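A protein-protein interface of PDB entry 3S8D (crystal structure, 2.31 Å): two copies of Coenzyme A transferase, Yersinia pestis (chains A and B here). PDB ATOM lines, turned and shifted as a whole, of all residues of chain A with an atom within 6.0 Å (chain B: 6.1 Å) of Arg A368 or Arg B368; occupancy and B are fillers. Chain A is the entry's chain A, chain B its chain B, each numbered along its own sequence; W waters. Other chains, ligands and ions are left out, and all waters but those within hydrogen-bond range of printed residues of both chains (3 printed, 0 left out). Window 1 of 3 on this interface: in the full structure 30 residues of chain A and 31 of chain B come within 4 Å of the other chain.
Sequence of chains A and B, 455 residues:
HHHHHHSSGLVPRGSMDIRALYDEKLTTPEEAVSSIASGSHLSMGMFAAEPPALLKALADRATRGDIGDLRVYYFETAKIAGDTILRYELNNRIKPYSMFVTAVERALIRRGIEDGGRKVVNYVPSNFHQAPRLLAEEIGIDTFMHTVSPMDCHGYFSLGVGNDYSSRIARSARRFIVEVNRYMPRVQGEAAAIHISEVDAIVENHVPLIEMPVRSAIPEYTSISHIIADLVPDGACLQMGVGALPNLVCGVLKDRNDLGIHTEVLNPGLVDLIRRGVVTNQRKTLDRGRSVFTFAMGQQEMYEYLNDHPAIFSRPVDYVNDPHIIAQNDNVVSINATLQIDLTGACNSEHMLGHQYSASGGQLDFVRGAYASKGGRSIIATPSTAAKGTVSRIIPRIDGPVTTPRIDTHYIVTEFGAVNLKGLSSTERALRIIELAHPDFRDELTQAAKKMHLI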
ATOM      1  N   ASN A 127       6.953  10.547 -19.169  1.00  0.00           N
ATOM      2  CA  ASN A 127       5.493  10.615 -19.090  1.00  0.00           C
ATOM      3  C   ASN A 127       4.995   9.596 -18.073  1.00  0.00           C
ATOM      4  O   ASN A 127       5.279   8.399 -18.204  1.00  0.00           O
ATOM      5  CB  ASN A 127       4.827  10.284 -20.428  1.00  0.00           C
ATOM      6  CG  ASN A 127       5.162  11.269 -21.508  1.00  0.00           C
ATOM      7  OD1 ASN A 127       4.687  12.409 -21.497  1.00  0.00           O
ATOM      8  ND2 ASN A 127       5.974  10.835 -22.469  1.00  0.00           N
ATOM      9  N   HIS A 129       2.126   8.281 -17.821  1.00  0.00           N
ATOM     10  CA  HIS A 129       1.376   7.209 -18.486  1.00  0.00           C
ATOM     11  C   HIS A 129       2.244   6.193 -19.269  1.00  0.00           C
ATOM     12  O   HIS A 129       1.741   5.160 -19.727  1.00  0.00           O
ATOM     13  CB  HIS A 129       0.267   7.764 -19.377  1.00  0.00           C
ATOM     14  CG  HIS A 129       0.774   8.388 -20.631  1.00  0.00           C
ATOM     15  ND1 HIS A 129       1.326   9.651 -20.657  1.00  0.00           N
ATOM     16  CD2 HIS A 129       0.834   7.920 -21.899  1.00  0.00           C
ATOM     17  CE1 HIS A 129       1.700   9.941 -21.891  1.00  0.00           C
ATOM     18  NE2 HIS A 129       1.412   8.907 -22.667  1.00  0.00           N
ATOM     19  N   GLN A 130       3.539   6.462 -19.382  1.00  0.00           N
ATOM     20  CA  GLN A 130       4.468   5.508 -19.995  1.00  0.00           C
ATOM     21  C   GLN A 130       5.362   4.818 -18.957  1.00  0.00           C
ATOM     22  O   GLN A 130       6.149   3.918 -19.295  1.00  0.00           O
ATOM     23  CB  GLN A 130       5.339   6.218 -21.025  1.00  0.00           C
ATOM     24  CG  GLN A 130       4.529   6.986 -22.067  1.00  0.00           C
ATOM     25  CD  GLN A 130       5.390   7.684 -23.104  1.00  0.00           C
ATOM     26  OE1 GLN A 130       6.520   8.100 -22.821  1.00  0.00           O
ATOM     27  NE2 GLN A 130       4.855   7.820 -24.313  1.00  0.00           N
ATOM     28  N   PRO A 323      -4.888   9.646 -23.102  1.00  0.00           N
ATOM     29  CA  PRO A 323      -5.864  10.636 -23.588  1.00  0.00           C
ATOM     30  C   PRO A 323      -6.933  10.006 -24.478  1.00  0.00           C
ATOM     31  O   PRO A 323      -8.091  10.475 -24.490  1.00  0.00           O
ATOM     32  CB  PRO A 323      -5.016  11.616 -24.411  1.00  0.00           C
ATOM     33  CG  PRO A 323      -3.582  11.416 -23.933  1.00  0.00           C
ATOM     34  CD  PRO A 323      -3.499   9.972 -23.483  1.00  0.00           C
ATOM     35  N   ALA A 327     -10.731  10.324 -23.397  1.00  0.00           N
ATOM     36  CA  ALA A 327     -11.691  10.959 -24.301  1.00  0.00           C
ATOM     37  C   ALA A 327     -12.875  10.063 -24.695  1.00  0.00           C
ATOM     38  O   ALA A 327     -13.807  10.524 -25.352  1.00  0.00           O
ATOM     39  CB  ALA A 327     -10.987  11.440 -25.543  1.00  0.00           C
ATOM     40  N   GLN A 363      -0.725  15.541 -15.397  1.00  0.00           N
ATOM     41  CA  GLN A 363      -2.019  16.183 -15.590  1.00  0.00           C
ATOM     42  C   GLN A 363      -2.229  16.592 -17.046  1.00  0.00           C
ATOM     43  O   GLN A 363      -3.360  16.804 -17.482  1.00  0.00           O
ATOM     44  CB  GLN A 363      -2.155  17.401 -14.676  1.00  0.00           C
ATOM     45  CG  GLN A 363      -1.876  17.110 -13.209  1.00  0.00           C
ATOM     46  CD  GLN A 363      -0.478  16.572 -12.973  1.00  0.00           C
ATOM     47  OE1 GLN A 363       0.465  16.927 -13.682  1.00  0.00           O
ATOM     48  NE2 GLN A 363      -0.336  15.710 -11.972  1.00  0.00           N
ATOM     49  N   LEU A 364      -1.136  16.698 -17.794  1.00  0.00           N
ATOM     50  CA  LEU A 364      -1.209  17.074 -19.201  1.00  0.00           C
ATOM     51  C   LEU A 364      -2.014  16.044 -19.985  1.00  0.00           C
ATOM     52  O   LEU A 364      -2.688  16.379 -20.959  1.00  0.00           O
ATOM     53  CB  LEU A 364       0.192  17.216 -19.797  1.00  0.00           C
ATOM     54  CG  LEU A 364       0.255  17.623 -21.270  1.00  0.00           C
ATOM     55  CD1 LEU A 364      -0.551  18.889 -21.513  1.00  0.00           C
ATOM     56  CD2 LEU A 364       1.695  17.804 -21.720  1.00  0.00           C
ATOM     57  N   ASP A 365      -1.939  14.790 -19.554  1.00  0.00           N
ATOM     58  CA  ASP A 365      -2.672  13.714 -20.205  1.00  0.00           C
ATOM     59  C   ASP A 365      -4.167  14.002 -20.150  1.00  0.00           C
ATOM     60  O   ASP A 365      -4.900  13.716 -21.095  1.00  0.00           O
ATOM     61  CB  ASP A 365      -2.373  12.375 -19.532  1.00  0.00           C
ATOM     62  CG  ASP A 365      -0.910  11.989 -19.625  1.00  0.00           C
ATOM     63  OD1 ASP A 365      -0.305  12.198 -20.697  1.00  0.00           O
ATOM     64  OD2 ASP A 365      -0.365  11.473 -18.627  1.00  0.00           O
ATOM     65  N   PHE A 366      -4.610  14.575 -19.035  1.00  0.00           N
ATOM     66  CA  PHE A 366      -6.023  14.909 -18.853  1.00  0.00           C
ATOM     67  C   PHE A 366      -6.409  16.206 -19.538  1.00  0.00           C
ATOM     68  O   PHE A 366      -7.491  16.306 -20.111  1.00  0.00           O
ATOM     69  CB  PHE A 366      -6.448  14.899 -17.368  1.00  0.00           C
ATOM     70  CG  PHE A 366      -6.742  13.524 -16.856  1.00  0.00           C
ATOM     71  CD1 PHE A 366      -8.022  12.993 -16.962  1.00  0.00           C
ATOM     72  CD2 PHE A 366      -5.724  12.737 -16.315  1.00  0.00           C
ATOM     73  CE1 PHE A 366      -8.291  11.712 -16.507  1.00  0.00           C
ATOM     74  CE2 PHE A 366      -5.976  11.459 -15.859  1.00  0.00           C
ATOM     75  CZ  PHE A 366      -7.250  10.936 -15.944  1.00  0.00           C
ATOM     76  N   VAL A 367      -5.527  17.193 -19.470  1.00  0.00           N
ATOM     77  CA  VAL A 367      -5.670  18.378 -20.316  1.00  0.00           C
ATOM     78  C   VAL A 367      -6.016  17.967 -21.754  1.00  0.00           C
ATOM     79  O   VAL A 367      -6.959  18.494 -22.356  1.00  0.00           O
ATOM     80  CB  VAL A 367      -4.398  19.243 -20.286  1.00  0.00           C
ATOM     81  CG1 VAL A 367      -4.445  20.320 -21.364  1.00  0.00           C
ATOM     82  CG2 VAL A 367      -4.230  19.883 -18.917  1.00  0.00           C
ATOM     83  N   ARG A 368      -5.283  16.999 -22.297  1.00  0.00           N
ATOM     84  CA  ARG A 368      -5.549  16.541 -23.668  1.00  0.00           C
ATOM     85  C   ARG A 368      -6.840  15.733 -23.769  1.00  0.00           C
ATOM     86  O   ARG A 368      -7.667  15.978 -24.666  1.00  0.00           O
ATOM     87  CB  ARG A 368      -4.387  15.712 -24.201  1.00  0.00           C
ATOM     88  CG  ARG A 368      -3.450  16.472 -25.098  1.00  0.00           C
ATOM     89  CD  ARG A 368      -2.201  16.855 -24.367  1.00  0.00           C
ATOM     90  NE  ARG A 368      -1.195  15.793 -24.360  1.00  0.00           N
ATOM     91  CZ  ARG A 368       0.099  15.987 -24.648  1.00  0.00           C
ATOM     92  NH1 ARG A 368       0.544  17.202 -24.982  1.00  0.00           N
ATOM     93  NH2 ARG A 368       0.957  14.964 -24.605  1.00  0.00           N
ATOM     94  N   GLY A 369      -7.003  14.768 -22.858  1.00  0.00           N
ATOM     95  CA  GLY A 369      -8.161  13.903 -22.875  1.00  0.00           C
ATOM     96  C   GLY A 369      -9.447  14.690 -22.730  1.00  0.00           C
ATOM     97  O   GLY A 369     -10.419  14.425 -23.445  1.00  0.00           O
ATOM     98  N   ALA A 370      -9.467  15.654 -21.810  1.00  0.00           N
ATOM     99  CA  ALA A 370     -10.709  16.375 -21.493  1.00  0.00           C
ATOM    100  C   ALA A 370     -11.223  17.133 -22.711  1.00  0.00           C
ATOM    101  O   ALA A 370     -12.429  17.154 -22.984  1.00  0.00           O
ATOM    102  CB  ALA A 370     -10.545  17.314 -20.273  1.00  0.00           C
ATOM    103  N   TYR A 371     -10.302  17.744 -23.453  1.00  0.00           N
ATOM    104  CA  TYR A 371     -10.682  18.478 -24.642  1.00  0.00           C
ATOM    105  C   TYR A 371     -11.131  17.517 -25.763  1.00  0.00           C
ATOM    106  O   TYR A 371     -12.087  17.798 -26.492  1.00  0.00           O
ATOM    107  CB  TYR A 371      -9.533  19.407 -25.078  1.00  0.00           C
ATOM    108  CG  TYR A 371      -9.872  20.315 -26.246  1.00  0.00           C
ATOM    109  CD1 TYR A 371     -10.744  21.394 -26.090  1.00  0.00           C
ATOM    110  CD2 TYR A 371      -9.314  20.098 -27.515  1.00  0.00           C
ATOM    111  CE1 TYR A 371     -11.060  22.237 -27.174  1.00  0.00           C
ATOM    112  CE2 TYR A 371      -9.619  20.927 -28.593  1.00  0.00           C
ATOM    113  CZ  TYR A 371     -10.488  22.001 -28.417  1.00  0.00           C
ATOM    114  OH  TYR A 371     -10.797  22.838 -29.479  1.00  0.00           O
ATOM    115  N   ALA A 372     -10.451  16.380 -25.893  1.00  0.00           N
ATOM    116  CA  ALA A 372     -10.862  15.369 -26.869  1.00  0.00           C
ATOM    117  C   ALA A 372     -12.231  14.743 -26.528  1.00  0.00           C
ATOM    118  O   ALA A 372     -12.964  14.322 -27.421  1.00  0.00           O
ATOM    119  CB  ALA A 372      -9.782  14.290 -27.009  1.00  0.00           C
ATOM    120  N   SER A 373     -12.561  14.674 -25.233  1.00  0.00           N
ATOM    121  CA  SER A 373     -13.871  14.188 -24.807  1.00  0.00           C
ATOM    122  C   SER A 373     -15.025  14.971 -25.447  1.00  0.00           C
ATOM    123  O   SER A 373     -14.961  16.191 -25.574  1.00  0.00           O
ATOM    124  CB  SER A 373     -14.006  14.262 -23.277  1.00  0.00           C
ATOM    125  OG  SER A 373     -15.318  13.902 -22.857  1.00  0.00           O
ATOM    126  N   SER A 378     -11.129  21.017 -20.077  1.00  0.00           N
ATOM    127  CA  SER A 378      -9.928  21.068 -19.279  1.00  0.00           C
ATOM    128  C   SER A 378      -9.926  22.434 -18.588  1.00  0.00           C
ATOM    129  O   SER A 378     -10.075  23.496 -19.239  1.00  0.00           O
ATOM    130  CB  SER A 378      -8.697  20.895 -20.167  1.00  0.00           C
ATOM    131  OG  SER A 378      -7.519  21.278 -19.476  1.00  0.00           O
ATOM    132  N   PRO A 405       1.740  23.439 -22.128  1.00  0.00           N
ATOM    133  CA  PRO A 405       2.047  24.341 -23.245  1.00  0.00           C
ATOM    134  C   PRO A 405       0.821  25.166 -23.652  1.00  0.00           C
ATOM    135  O   PRO A 405      -0.316  24.803 -23.292  1.00  0.00           O
ATOM    136  CB  PRO A 405       2.434  23.383 -24.390  1.00  0.00           C
ATOM    137  CG  PRO A 405       2.688  22.067 -23.744  1.00  0.00           C
ATOM    138  CD  PRO A 405       1.830  22.022 -22.517  1.00  0.00           C
ATOM    139  N   ASP A 408      -2.096  23.519 -25.719  1.00  0.00           N
ATOM    140  CA  ASP A 408      -2.930  22.543 -25.022  1.00  0.00           C
ATOM    141  C   ASP A 408      -3.959  23.167 -24.088  1.00  0.00           C
ATOM    142  O   ASP A 408      -5.017  22.604 -23.857  1.00  0.00           O
ATOM    143  CB  ASP A 408      -2.054  21.572 -24.230  1.00  0.00           C
ATOM    144  CG  ASP A 408      -1.278  20.643 -25.127  1.00  0.00           C
ATOM    145  OD1 ASP A 408      -1.894  20.078 -26.065  1.00  0.00           O
ATOM    146  OD2 ASP A 408      -0.057  20.496 -24.907  1.00  0.00           O
ATOM    147  N   ASN B 127      -2.696  23.039 -32.170  1.00  0.00           N
ATOM    148  CA  ASN B 127      -2.370  21.702 -32.636  1.00  0.00           C
ATOM    149  C   ASN B 127      -2.853  21.489 -34.074  1.00  0.00           C
ATOM    150  O   ASN B 127      -4.062  21.574 -34.345  1.00  0.00           O
ATOM    151  CB  ASN B 127      -3.019  20.668 -31.709  1.00  0.00           C
ATOM    152  CG  ASN B 127      -2.282  20.519 -30.401  1.00  0.00           C
ATOM    153  OD1 ASN B 127      -1.306  19.766 -30.315  1.00  0.00           O
ATOM    154  ND2 ASN B 127      -2.741  21.232 -29.366  1.00  0.00           N
ATOM    155  N   HIS B 129      -3.305  18.843 -35.674  1.00  0.00           N
ATOM    156  CA  HIS B 129      -4.326  17.787 -35.678  1.00  0.00           C
ATOM    157  C   HIS B 129      -5.689  18.229 -35.091  1.00  0.00           C
ATOM    158  O   HIS B 129      -6.710  17.563 -35.283  1.00  0.00           O
ATOM    159  CB  HIS B 129      -3.818  16.546 -34.955  1.00  0.00           C
ATOM    160  CG  HIS B 129      -3.946  16.628 -33.468  1.00  0.00           C
ATOM    161  ND1 HIS B 129      -3.072  17.357 -32.685  1.00  0.00           N
ATOM    162  CD2 HIS B 129      -4.848  16.075 -32.617  1.00  0.00           C
ATOM    163  CE1 HIS B 129      -3.425  17.245 -31.413  1.00  0.00           C
ATOM    164  NE2 HIS B 129      -4.501  16.475 -31.343  1.00  0.00           N
ATOM    165  N   GLN B 130      -5.702  19.353 -34.387  1.00  0.00           N
ATOM    166  CA  GLN B 130      -6.951  19.941 -33.919  1.00  0.00           C
ATOM    167  C   GLN B 130      -7.475  21.056 -34.858  1.00  0.00           C
ATOM    168  O   GLN B 130      -8.552  21.632 -34.639  1.00  0.00           O
ATOM    169  CB  GLN B 130      -6.743  20.471 -32.507  1.00  0.00           C
ATOM    170  CG  GLN B 130      -6.463  19.345 -31.476  1.00  0.00           C
ATOM    171  CD  GLN B 130      -6.241  19.846 -30.039  1.00  0.00           C
ATOM    172  OE1 GLN B 130      -6.168  21.055 -29.774  1.00  0.00           O
ATOM    173  NE2 GLN B 130      -6.126  18.905 -29.107  1.00  0.00           N
ATOM    174  N   PRO B 323      -2.200  10.517 -32.745  1.00  0.00           N
ATOM    175  CA  PRO B 323      -1.220   9.500 -32.334  1.00  0.00           C
ATOM    176  C   PRO B 323      -1.888   8.151 -32.085  1.00  0.00           C
ATOM    177  O   PRO B 323      -1.247   7.103 -32.253  1.00  0.00           O
ATOM    178  CB  PRO B 323      -0.669  10.036 -31.000  1.00  0.00           C
ATOM    179  CG  PRO B 323      -1.107  11.495 -30.930  1.00  0.00           C
ATOM    180  CD  PRO B 323      -2.387  11.572 -31.731  1.00  0.00           C
ATOM    181  N   ALA B 327      -0.332   4.992 -33.958  1.00  0.00           N
ATOM    182  CA  ALA B 327       0.047   3.848 -33.110  1.00  0.00           C
ATOM    183  C   ALA B 327      -0.546   2.506 -33.544  1.00  0.00           C
ATOM    184  O   ALA B 327      -0.004   1.444 -33.209  1.00  0.00           O
ATOM    185  CB  ALA B 327      -0.364   4.113 -31.652  1.00  0.00           C
ATOM    186  N   GLN B 363       4.678  17.544 -36.282  1.00  0.00           N
ATOM    187  CA  GLN B 363       5.607  16.424 -36.245  1.00  0.00           C
ATOM    188  C   GLN B 363       5.653  15.796 -34.856  1.00  0.00           C
ATOM    189  O   GLN B 363       6.058  14.645 -34.699  1.00  0.00           O
ATOM    190  CB  GLN B 363       7.006  16.872 -36.674  1.00  0.00           C
ATOM    191  CG  GLN B 363       7.114  17.240 -38.147  1.00  0.00           C
ATOM    192  CD  GLN B 363       6.568  18.623 -38.445  1.00  0.00           C
ATOM    193  OE1 GLN B 363       7.227  19.631 -38.194  1.00  0.00           O
ATOM    194  NE2 GLN B 363       5.356  18.678 -38.986  1.00  0.00           N
ATOM    195  N   LEU B 364       5.234  16.558 -33.852  1.00  0.00           N
ATOM    196  CA  LEU B 364       5.220  16.064 -32.481  1.00  0.00           C
ATOM    197  C   LEU B 364       4.191  14.951 -32.341  1.00  0.00           C
ATOM    198  O   LEU B 364       4.370  14.021 -31.556  1.00  0.00           O
ATOM    199  CB  LEU B 364       4.912  17.194 -31.499  1.00  0.00           C
ATOM    200  CG  LEU B 364       4.690  16.769 -30.047  1.00  0.00           C
ATOM    201  CD1 LEU B 364       5.905  16.029 -29.510  1.00  0.00           C
ATOM    202  CD2 LEU B 364       4.365  17.972 -29.177  1.00  0.00           C
ATOM    203  N   ASP B 365       3.114  15.054 -33.112  1.00  0.00           N
ATOM    204  CA  ASP B 365       2.059  14.052 -33.087  1.00  0.00           C
ATOM    205  C   ASP B 365       2.621  12.696 -33.491  1.00  0.00           C
ATOM    206  O   ASP B 365       2.217  11.663 -32.958  1.00  0.00           O
ATOM    207  CB  ASP B 365       0.916  14.448 -34.023  1.00  0.00           C
ATOM    208  CG  ASP B 365       0.142  15.651 -33.521  1.00  0.00           C
ATOM    209  OD1 ASP B 365      -0.203  15.683 -32.321  1.00  0.00           O
ATOM    210  OD2 ASP B 365      -0.124  16.566 -34.328  1.00  0.00           O
ATOM    211  N   PHE B 366       3.556  12.704 -34.436  1.00  0.00           N
ATOM    212  CA  PHE B 366       4.171  11.466 -34.902  1.00  0.00           C
ATOM    213  C   PHE B 366       5.207  10.951 -33.908  1.00  0.00           C
ATOM    214  O   PHE B 366       5.322   9.744 -33.700  1.00  0.00           O
ATOM    215  CB  PHE B 366       4.747  11.627 -36.309  1.00  0.00           C
ATOM    216  CG  PHE B 366       3.741  11.378 -37.393  1.00  0.00           C
ATOM    217  CD1 PHE B 366       3.608  10.123 -37.960  1.00  0.00           C
ATOM    218  CD2 PHE B 366       2.909  12.395 -37.830  1.00  0.00           C
ATOM    219  CE1 PHE B 366       2.675   9.889 -38.951  1.00  0.00           C
ATOM    220  CE2 PHE B 366       1.974  12.168 -38.821  1.00  0.00           C
ATOM    221  CZ  PHE B 366       1.859  10.913 -39.382  1.00  0.00           C
ATOM    222  N   VAL B 367       5.951  11.860 -33.283  1.00  0.00           N
ATOM    223  CA  VAL B 367       6.894  11.448 -32.260  1.00  0.00           C
ATOM    224  C   VAL B 367       6.186  10.549 -31.241  1.00  0.00           C
ATOM    225  O   VAL B 367       6.706   9.477 -30.886  1.00  0.00           O
ATOM    226  CB  VAL B 367       7.536  12.661 -31.569  1.00  0.00           C
ATOM    227  CG1 VAL B 367       8.462  12.206 -30.431  1.00  0.00           C
ATOM    228  CG2 VAL B 367       8.291  13.510 -32.595  1.00  0.00           C
ATOM    229  N   ARG B 368       5.007  10.968 -30.776  1.00  0.00           N
ATOM    230  CA  ARG B 368       4.269  10.177 -29.784  1.00  0.00           C
ATOM    231  C   ARG B 368       3.650   8.930 -30.433  1.00  0.00           C
ATOM    232  O   ARG B 368       3.796   7.806 -29.924  1.00  0.00           O
ATOM    233  CB  ARG B 368       3.189  11.016 -29.092  1.00  0.00           C
ATOM    234  CG  ARG B 368       3.727  12.338 -28.540  1.00  0.00           C
ATOM    235  CD  ARG B 368       2.811  13.015 -27.543  1.00  0.00           C
ATOM    236  NE  ARG B 368       1.798  13.869 -28.160  1.00  0.00           N
ATOM    237  CZ  ARG B 368       1.602  15.149 -27.833  1.00  0.00           C
ATOM    238  NH1 ARG B 368       2.359  15.738 -26.898  1.00  0.00           N
ATOM    239  NH2 ARG B 368       0.648  15.848 -28.440  1.00  0.00           N
ATOM    240  N   GLY B 369       2.971   9.127 -31.560  1.00  0.00           N
ATOM    241  CA  GLY B 369       2.380   8.010 -32.270  1.00  0.00           C
ATOM    242  C   GLY B 369       3.392   6.921 -32.575  1.00  0.00           C
ATOM    243  O   GLY B 369       3.098   5.736 -32.419  1.00  0.00           O
ATOM    244  N   ALA B 370       4.587   7.309 -33.007  1.00  0.00           N
ATOM    245  CA  ALA B 370       5.597   6.324 -33.393  1.00  0.00           C
ATOM    246  C   ALA B 370       6.122   5.500 -32.192  1.00  0.00           C
ATOM    247  O   ALA B 370       6.338   4.291 -32.298  1.00  0.00           O
ATOM    248  CB  ALA B 370       6.741   7.008 -34.129  1.00  0.00           C
ATOM    249  N   TYR B 371       6.328   6.147 -31.054  1.00  0.00           N
ATOM    250  CA  TYR B 371       6.696   5.400 -29.852  1.00  0.00           C
ATOM    251  C   TYR B 371       5.566   4.467 -29.360  1.00  0.00           C
ATOM    252  O   TYR B 371       5.834   3.385 -28.855  1.00  0.00           O
ATOM    253  CB  TYR B 371       7.144   6.351 -28.738  1.00  0.00           C
ATOM    254  CG  TYR B 371       7.709   5.659 -27.515  1.00  0.00           C
ATOM    255  CD1 TYR B 371       8.878   4.915 -27.600  1.00  0.00           C
ATOM    256  CD2 TYR B 371       7.082   5.767 -26.260  1.00  0.00           C
ATOM    257  CE1 TYR B 371       9.417   4.279 -26.480  1.00  0.00           C
ATOM    258  CE2 TYR B 371       7.612   5.132 -25.132  1.00  0.00           C
ATOM    259  CZ  TYR B 371       8.786   4.394 -25.252  1.00  0.00           C
ATOM    260  OH  TYR B 371       9.344   3.769 -24.157  1.00  0.00           O
ATOM    261  N   ALA B 372       4.309   4.879 -29.506  1.00  0.00           N
ATOM    262  CA  ALA B 372       3.199   4.027 -29.084  1.00  0.00           C
ATOM    263  C   ALA B 372       2.997   2.841 -30.047  1.00  0.00           C
ATOM    264  O   ALA B 372       2.458   1.796 -29.679  1.00  0.00           O
ATOM    265  CB  ALA B 372       1.919   4.842 -28.940  1.00  0.00           C
ATOM    266  N   SER B 373       3.454   3.004 -31.277  1.00  0.00           N
ATOM    267  CA  SER B 373       3.372   1.935 -32.255  1.00  0.00           C
ATOM    268  C   SER B 373       4.176   0.708 -31.804  1.00  0.00           C
ATOM    269  O   SER B 373       5.333   0.830 -31.369  1.00  0.00           O
ATOM    270  CB  SER B 373       3.897   2.426 -33.612  1.00  0.00           C
ATOM    271  OG  SER B 373       3.994   1.356 -34.541  1.00  0.00           O
ATOM    272  N   SER B 378      10.332   6.855 -33.127  1.00  0.00           N
ATOM    273  CA  SER B 378      10.410   8.245 -33.528  1.00  0.00           C
ATOM    274  C   SER B 378      11.889   8.636 -33.680  1.00  0.00           C
ATOM    275  O   SER B 378      12.702   8.479 -32.743  1.00  0.00           O
ATOM    276  CB  SER B 378       9.715   9.147 -32.500  1.00  0.00           C
ATOM    277  OG  SER B 378      10.085  10.491 -32.725  1.00  0.00           O
ATOM    278  N   PRO B 405       9.380  18.221 -26.543  1.00  0.00           N
ATOM    279  CA  PRO B 405       9.716  18.192 -25.118  1.00  0.00           C
ATOM    280  C   PRO B 405      10.684  17.054 -24.881  1.00  0.00           C
ATOM    281  O   PRO B 405      10.652  16.078 -25.642  1.00  0.00           O
ATOM    282  CB  PRO B 405       8.369  17.882 -24.452  1.00  0.00           C
ATOM    283  CG  PRO B 405       7.342  18.418 -25.429  1.00  0.00           C
ATOM    284  CD  PRO B 405       7.925  18.134 -26.784  1.00  0.00           C
ATOM    285  N   ASP B 408       9.272  13.464 -24.513  1.00  0.00           N
ATOM    286  CA  ASP B 408       8.741  12.776 -25.689  1.00  0.00           C
ATOM    287  C   ASP B 408       9.819  12.203 -26.585  1.00  0.00           C
ATOM    288  O   ASP B 408       9.648  11.154 -27.193  1.00  0.00           O
ATOM    289  CB  ASP B 408       7.813  13.692 -26.487  1.00  0.00           C
ATOM    290  CG  ASP B 408       6.554  14.048 -25.708  1.00  0.00           C
ATOM    291  OD1 ASP B 408       5.990  13.143 -25.045  1.00  0.00           O
ATOM    292  OD2 ASP B 408       6.132  15.227 -25.738  1.00  0.00           O
HETATM  293  O   HOH W   1      -1.796  17.924 -27.731  1.00  0.00           O
HETATM  294  O   HOH W   2      -4.662  19.801 -26.868  1.00  0.00           O
HETATM  295  O   HOH W   3       3.256  12.587 -24.453  1.00  0.00           O
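The side-chain amide nitrogen (ND2) of Asn A127 is in hydrogen-bond range of the side-chain carboxylate (OD1) of Asp B408.
The guanidinium group of Arg A368 lies close to the guanidinium group of Arg B368, at 2.8 Å.
The side-chain amide nitrogen (ND2) of Asn A127 is in hydrogen-bond range of the side-chain amide oxygen (OE1) of Gln A130 (2.8 Å).
The guanidinium group (NH1) of Arg A368 is in salt-bridge range of the side-chain carboxylate (OD2) of Asp A408, at 3.3 Å.
The side-chain amide oxygen (OE1) of Gln B130 is in hydrogen-bond range of the side-chain amide nitrogen (ND2) of Asn B127 (3.5 Å).
The side-chain carboxylate (OD1) of Asp B365 is in salt-bridge range of the guanidinium group (NH2) of Arg B368 (3.98 Å).
OD2 of Asp B408 is in salt-bridge range of NH1 of Arg B368 (3.98 Å).
Among the printed residues, pairs that only touch across the chains: Asp A408 with Asn B127, Gln A130 with Tyr B371 and Tyr A371 with Gln B130.
Ala A327 touches none of the printed residues of chain B.
Of the printed residues of chain B, Asp A408 touches Asn B127 (3.6 Å).
Of the printed residues of chain A, Asn B127 touches Asp A408 (3.6 Å).
Pro B323 touches none of the printed residues of chain A.
Arg B368 touches just one residue of chain A: Arg A368.
Printed residues of chain A within 4 Å of Tyr B371: Gln A130.
Printed residues of chain A within 4 Å of Asp B408: Asn A127 (3.5 Å).
The nearest residue of chain B that does not touch Arg A368 is Asp B408 (5.3 Å).
Hydrophobic or aromatic side chains of chain B that line the printed part of chain A: Tyr B371.
Hydrophobic or aromatic side chains of chain A within 4 Å of the printed part of chain B: Tyr A371.
Asn A127 touches Asp B408, and with the chains exchanged Asp A408 touches Asn B127.
Gln A130 touches Tyr B371, and with the chains exchanged Tyr A371 touches Gln B130.
Arg B368 touches its own counterpart, Arg A368.
19 positions are printed for both chains.
Of the 5 pairs that touch across the chains among the printed residues, 5 have their exchanged pair printed and touching as well.
Water W1 lies within hydrogen-bond range of the side-chain carboxylate of Asp A408, the side-chain amide oxygen of Asn B127 and the guanidinium group of Arg B368.
Water W2 lies within hydrogen-bond range of NE2 of Gln B130, OD1 of Asp A408 and ND2 of Asn B127.
Water W3 lies within hydrogen-bond range of the side-chain carboxylate (OD1) of Asp B408, the side-chain amide oxygen (OD1) of Asn A127 and the guanidinium group (NH2) of Arg A368.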
